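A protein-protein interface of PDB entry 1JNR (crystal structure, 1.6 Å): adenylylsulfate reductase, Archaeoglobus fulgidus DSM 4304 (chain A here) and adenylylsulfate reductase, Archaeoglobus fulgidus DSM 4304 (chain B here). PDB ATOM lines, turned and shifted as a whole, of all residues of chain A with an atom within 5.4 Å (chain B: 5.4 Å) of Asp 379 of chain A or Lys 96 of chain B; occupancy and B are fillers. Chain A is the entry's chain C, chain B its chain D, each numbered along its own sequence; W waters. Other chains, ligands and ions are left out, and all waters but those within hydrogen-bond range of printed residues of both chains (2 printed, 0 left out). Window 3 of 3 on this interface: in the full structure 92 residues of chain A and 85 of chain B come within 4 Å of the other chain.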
ATOM      1  N   TYR A 355      -1.453   5.526   3.045  1.00  0.00           N
ATOM      2  CA  TYR A 355      -2.697   6.280   3.182  1.00  0.00           C
ATOM      3  C   TYR A 355      -2.555   7.164   4.419  1.00  0.00           C
ATOM      4  O   TYR A 355      -2.939   8.336   4.416  1.00  0.00           O
ATOM      5  CB  TYR A 355      -3.866   5.315   3.376  1.00  0.00           C
ATOM      6  CG  TYR A 355      -5.237   5.946   3.314  1.00  0.00           C
ATOM      7  CD1 TYR A 355      -5.774   6.371   2.101  1.00  0.00           C
ATOM      8  CD2 TYR A 355      -6.023   6.067   4.460  1.00  0.00           C
ATOM      9  CE1 TYR A 355      -7.061   6.891   2.025  1.00  0.00           C
ATOM     10  CE2 TYR A 355      -7.314   6.589   4.396  1.00  0.00           C
ATOM     11  CZ  TYR A 355      -7.827   6.995   3.172  1.00  0.00           C
ATOM     12  OH  TYR A 355      -9.115   7.473   3.088  1.00  0.00           O
ATOM     13  N   ASN A 377     -16.732  14.777   1.011  1.00  0.00           N
ATOM     14  CA  ASN A 377     -16.709  13.321   0.904  1.00  0.00           C
ATOM     15  C   ASN A 377     -15.717  12.807  -0.127  1.00  0.00           C
ATOM     16  O   ASN A 377     -16.035  11.930  -0.930  1.00  0.00           O
ATOM     17  CB  ASN A 377     -18.105  12.784   0.579  1.00  0.00           C
ATOM     18  CG  ASN A 377     -19.068  12.961   1.729  1.00  0.00           C
ATOM     19  OD1 ASN A 377     -18.681  12.846   2.890  1.00  0.00           O
ATOM     20  ND2 ASN A 377     -20.333  13.230   1.417  1.00  0.00           N
ATOM     21  N   ILE A 378     -14.508  13.352  -0.097  1.00  0.00           N
ATOM     22  CA  ILE A 378     -13.473  12.933  -1.026  1.00  0.00           C
ATOM     23  C   ILE A 378     -12.481  12.001  -0.340  1.00  0.00           C
ATOM     24  O   ILE A 378     -11.799  12.391   0.607  1.00  0.00           O
ATOM     25  CB  ILE A 378     -12.702  14.147  -1.594  1.00  0.00           C
ATOM     26  CG1 ILE A 378     -13.649  15.021  -2.421  1.00  0.00           C
ATOM     27  CG2 ILE A 378     -11.527  13.671  -2.441  1.00  0.00           C
ATOM     28  CD1 ILE A 378     -13.019  16.313  -2.913  1.00  0.00           C
ATOM     29  N   ASP A 379     -12.434  10.760  -0.812  1.00  0.00           N
ATOM     30  CA  ASP A 379     -11.508   9.764  -0.292  1.00  0.00           C
ATOM     31  C   ASP A 379     -10.426   9.663  -1.361  1.00  0.00           C
ATOM     32  O   ASP A 379     -10.677   9.177  -2.464  1.00  0.00           O
ATOM     33  CB  ASP A 379     -12.214   8.421  -0.115  1.00  0.00           C
ATOM     34  CG  ASP A 379     -11.284   7.344   0.396  1.00  0.00           C
ATOM     35  OD1 ASP A 379     -11.771   6.237   0.709  1.00  0.00           O
ATOM     36  OD2 ASP A 379     -10.063   7.605   0.480  1.00  0.00           O
ATOM     37  N   PRO A 380      -9.203  10.121  -1.046  1.00  0.00           N
ATOM     38  CA  PRO A 380      -8.087  10.091  -1.997  1.00  0.00           C
ATOM     39  C   PRO A 380      -7.744   8.755  -2.650  1.00  0.00           C
ATOM     40  O   PRO A 380      -7.127   8.729  -3.716  1.00  0.00           O
ATOM     41  CB  PRO A 380      -6.929  10.671  -1.185  1.00  0.00           C
ATOM     42  CG  PRO A 380      -7.261  10.254   0.217  1.00  0.00           C
ATOM     43  CD  PRO A 380      -8.741  10.532   0.293  1.00  0.00           C
ATOM     44  N   GLN A 381      -8.128   7.651  -2.018  1.00  0.00           N
ATOM     45  CA  GLN A 381      -7.847   6.337  -2.588  1.00  0.00           C
ATOM     46  C   GLN A 381      -8.898   5.971  -3.633  1.00  0.00           C
ATOM     47  O   GLN A 381      -8.702   5.048  -4.420  1.00  0.00           O
ATOM     48  CB  GLN A 381      -7.835   5.265  -1.493  1.00  0.00           C
ATOM     49  CG  GLN A 381      -9.158   5.134  -0.762  1.00  0.00           C
ATOM     50  CD  GLN A 381      -9.147   4.060   0.308  1.00  0.00           C
ATOM     51  OE1 GLN A 381      -9.985   4.066   1.210  1.00  0.00           O
ATOM     52  NE2 GLN A 381      -8.207   3.126   0.209  1.00  0.00           N
ATOM     53  N   GLU A 382     -10.009   6.703  -3.643  1.00  0.00           N
ATOM     54  CA  GLU A 382     -11.090   6.425  -4.582  1.00  0.00           C
ATOM     55  C   GLU A 382     -11.228   7.427  -5.725  1.00  0.00           C
ATOM     56  O   GLU A 382     -11.417   7.038  -6.877  1.00  0.00           O
ATOM     57  CB  GLU A 382     -12.418   6.314  -3.827  1.00  0.00           C
ATOM     58  CG  GLU A 382     -12.461   5.143  -2.856  1.00  0.00           C
ATOM     59  CD  GLU A 382     -12.309   3.797  -3.553  1.00  0.00           C
ATOM     60  OE1 GLU A 382     -12.129   2.781  -2.849  1.00  0.00           O
ATOM     61  OE2 GLU A 382     -12.377   3.754  -4.801  1.00  0.00           O
ATOM     62  N   GLN A 383     -11.148   8.715  -5.420  1.00  0.00           N
ATOM     63  CA  GLN A 383     -11.265   9.711  -6.473  1.00  0.00           C
ATOM     64  C   GLN A 383     -10.199  10.785  -6.389  1.00  0.00           C
ATOM     65  O   GLN A 383      -9.660  11.054  -5.319  1.00  0.00           O
ATOM     66  CB  GLN A 383     -12.657  10.358  -6.456  1.00  0.00           C
ATOM     67  CG  GLN A 383     -13.139  10.854  -5.098  1.00  0.00           C
ATOM     68  CD  GLN A 383     -13.790   9.759  -4.275  1.00  0.00           C
ATOM     69  OE1 GLN A 383     -14.561   8.953  -4.798  1.00  0.00           O
ATOM     70  NE2 GLN A 383     -13.499   9.733  -2.980  1.00  0.00           N
ATOM     71  N   VAL B  90     -10.913  12.320  11.760  1.00  0.00           N
ATOM     72  CA  VAL B  90     -11.453  13.042  10.621  1.00  0.00           C
ATOM     73  C   VAL B  90     -12.824  12.460  10.356  1.00  0.00           C
ATOM     74  O   VAL B  90     -12.959  11.266  10.079  1.00  0.00           O
ATOM     75  CB  VAL B  90     -10.569  12.867   9.377  1.00  0.00           C
ATOM     76  CG1 VAL B  90     -11.168  13.631   8.197  1.00  0.00           C
ATOM     77  CG2 VAL B  90      -9.167  13.378   9.675  1.00  0.00           C
ATOM     78  N   LYS B  91     -13.843  13.304  10.469  1.00  0.00           N
ATOM     79  CA  LYS B  91     -15.205  12.861  10.248  1.00  0.00           C
ATOM     80  C   LYS B  91     -15.777  13.461   8.973  1.00  0.00           C
ATOM     81  O   LYS B  91     -15.847  14.682   8.817  1.00  0.00           O
ATOM     82  CB  LYS B  91     -16.081  13.226  11.443  1.00  0.00           C
ATOM     83  CG  LYS B  91     -17.477  12.612  11.352  1.00  0.00           C
ATOM     84  CD  LYS B  91     -18.272  12.782  12.633  1.00  0.00           C
ATOM     85  CE  LYS B  91     -19.513  11.893  12.621  1.00  0.00           C
ATOM     86  NZ  LYS B  91     -20.230  11.890  13.937  1.00  0.00           N
ATOM     87  N   TYR B  92     -16.183  12.578   8.068  1.00  0.00           N
ATOM     88  CA  TYR B  92     -16.747  12.961   6.783  1.00  0.00           C
ATOM     89  C   TYR B  92     -18.215  13.340   6.867  1.00  0.00           C
ATOM     90  O   TYR B  92     -18.932  12.920   7.777  1.00  0.00           O
ATOM     91  CB  TYR B  92     -16.592  11.807   5.789  1.00  0.00           C
ATOM     92  CG  TYR B  92     -15.246  11.747   5.111  1.00  0.00           C
ATOM     93  CD1 TYR B  92     -14.063  11.843   5.844  1.00  0.00           C
ATOM     94  CD2 TYR B  92     -15.153  11.604   3.728  1.00  0.00           C
ATOM     95  CE1 TYR B  92     -12.823  11.803   5.215  1.00  0.00           C
ATOM     96  CE2 TYR B  92     -13.923  11.562   3.087  1.00  0.00           C
ATOM     97  CZ  TYR B  92     -12.761  11.664   3.835  1.00  0.00           C
ATOM     98  OH  TYR B  92     -11.541  11.638   3.202  1.00  0.00           O
ATOM     99  N   ASN B  94     -20.445  12.278   5.075  1.00  0.00           N
ATOM    100  CA  ASN B  94     -21.219  11.047   4.926  1.00  0.00           C
ATOM    101  C   ASN B  94     -21.163  10.114   6.131  1.00  0.00           C
ATOM    102  O   ASN B  94     -21.718   9.011   6.094  1.00  0.00           O
ATOM    103  CB  ASN B  94     -20.799  10.282   3.662  1.00  0.00           C
ATOM    104  CG  ASN B  94     -19.364   9.788   3.711  1.00  0.00           C
ATOM    105  OD1 ASN B  94     -18.791   9.595   4.782  1.00  0.00           O
ATOM    106  ND2 ASN B  94     -18.783   9.553   2.539  1.00  0.00           N
ATOM    107  N   GLY B  95     -20.498  10.549   7.196  1.00  0.00           N
ATOM    108  CA  GLY B  95     -20.423   9.734   8.398  1.00  0.00           C
ATOM    109  C   GLY B  95     -19.151   8.933   8.589  1.00  0.00           C
ATOM    110  O   GLY B  95     -18.892   8.429   9.683  1.00  0.00           O
ATOM    111  N   LYS B  96     -18.359   8.801   7.531  1.00  0.00           N
ATOM    112  CA  LYS B  96     -17.110   8.059   7.614  1.00  0.00           C
ATOM    113  C   LYS B  96     -16.218   8.689   8.674  1.00  0.00           C
ATOM    114  O   LYS B  96     -16.204   9.909   8.838  1.00  0.00           O
ATOM    115  CB  LYS B  96     -16.393   8.086   6.268  1.00  0.00           C
ATOM    116  CG  LYS B  96     -15.088   7.322   6.244  1.00  0.00           C
ATOM    117  CD  LYS B  96     -14.469   7.374   4.860  1.00  0.00           C
ATOM    118  CE  LYS B  96     -13.284   6.438   4.753  1.00  0.00           C
ATOM    119  NZ  LYS B  96     -12.774   6.383   3.360  1.00  0.00           N
ATOM    120  N   VAL B  97     -15.481   7.856   9.400  1.00  0.00           N
ATOM    121  CA  VAL B  97     -14.582   8.352  10.433  1.00  0.00           C
ATOM    122  C   VAL B  97     -13.200   7.738  10.276  1.00  0.00           C
ATOM    123  O   VAL B  97     -13.055   6.520  10.194  1.00  0.00           O
ATOM    124  CB  VAL B  97     -15.112   8.032  11.848  1.00  0.00           C
ATOM    125  CG1 VAL B  97     -14.132   8.536  12.900  1.00  0.00           C
ATOM    126  CG2 VAL B  97     -16.468   8.680  12.049  1.00  0.00           C
ATOM    127  N   LEU B  98     -12.188   8.596  10.217  1.00  0.00           N
ATOM    128  CA  LEU B  98     -10.809   8.149  10.087  1.00  0.00           C
ATOM    129  C   LEU B  98     -10.073   8.570  11.349  1.00  0.00           C
ATOM    130  O   LEU B  98     -10.358   9.625  11.917  1.00  0.00           O
ATOM    131  CB  LEU B  98     -10.141   8.795   8.870  1.00  0.00           C
ATOM    132  CG  LEU B  98     -10.751   8.525   7.492  1.00  0.00           C
ATOM    133  CD1 LEU B  98      -9.990   9.320   6.441  1.00  0.00           C
ATOM    134  CD2 LEU B  98     -10.696   7.034   7.180  1.00  0.00           C
HETATM  135  O   HOH W   1     -10.437   5.305   4.374  1.00  0.00           O
HETATM  136  O   HOH W   2     -14.446   5.618   0.511  1.00  0.00           O
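Of the 8 printed residues of chain B, 4 touch a printed residue of chain A. Hydrophobic or aromatic side chains of chain B within 4 Å of the printed part of chain A: Tyr 92 and Leu 98. Of the 8 printed residues of chain A, 4 touch a printed residue of chain B. Printed residues of chain A that touch a printed residue of chain B: Tyr 355, Asn 377, Ile 378 and Asp 379. Among the printed residues, 7 pairs touch across the chains. Among the printed residues, Asp or Glu carboxylates within 4 Å of a Lys or Arg side-chain nitrogen of the other chain: Asp 379 of chain A with Lys 96 of chain B.
The backbone carbonyl oxygen of Leu 98 of chain B is in hydrogen-bond range of the backbone NH of Val 90 of chain B, 2.8 Å away. The backbone NH of Lys 96 of chain B sits at hydrogen-bond distance from the side-chain amide oxygen of Asn 94 of chain B (2.9 Å). The backbone NH (N) of Asp 379 of chain A sits close to the side-chain amide nitrogen (NE2) of Gln 383 of chain A, 2.6 Å away. The side-chain carboxylate (OD2) of Asp 379 of chain A is in hydrogen-bond range of the side-chain hydroxyl (OH) of Tyr 355 of chain A (2.8 Å). The side-chain amide oxygen (OE1) of Gln 381 of chain A sits close to the side-chain carboxylate (OD1) of Asp 379 of chain A.
Water W2 bridges the side-chain carboxylate of Asp 379 of chain A (2.8 Å) and the side-chain amino group of Lys 96 of chain B (3.4 Å). Water W1 lies within hydrogen-bond range of the side-chain amino group (NZ) of Lys 96 of chain B (2.8 Å), the side-chain hydroxyl (OH) of Tyr 355 of chain A (2.8 Å) and the side-chain amide oxygen (OE1) of Gln 381 of chain A (3.4 Å).
Of the printed residues of chain B, Asp 379 of chain A touches Tyr 92 and Lys 96. Lys 96 of chain B touches just these residues of chain A: Tyr 355 (3.8 Å) and Asp 379 (2.8 Å). Of the printed residues of chain B, Tyr 355 of chain A touches Lys 96 and Leu 98. Of the printed residues of chain A, Leu 98 of chain B touches Tyr 355 (3.9 Å). Printed residues of chain A within 4 Å of Asn 94 of chain B: Asn 377 (2.9 Å).
The side-chain amide oxygen (OD1) of Asn 377 of chain A sits at hydrogen-bond distance from the backbone NH (N) of Asn 94 of chain B (2.9 Å). The backbone carbonyl oxygen (O) of Ile 378 of chain A is in hydrogen-bond range of the side-chain hydroxyl (OH) of Tyr 92 of chain B, 2.7 Å away. The side-chain carboxylate (OD1) of Asp 379 of chain A lies within salt-bridge range of the side-chain amino group (NZ) of Lys 96 of chain B (2.8 Å).
Among the printed residues, merely in contact across the chains: Tyr 355 of chain A with Lys 96 of chain B, Tyr 355 of chain A with Leu 98 of chain B, Asn 377 of chain A with Tyr 92 of chain B and Asp 379 of chain A with Tyr 92 of chain B.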
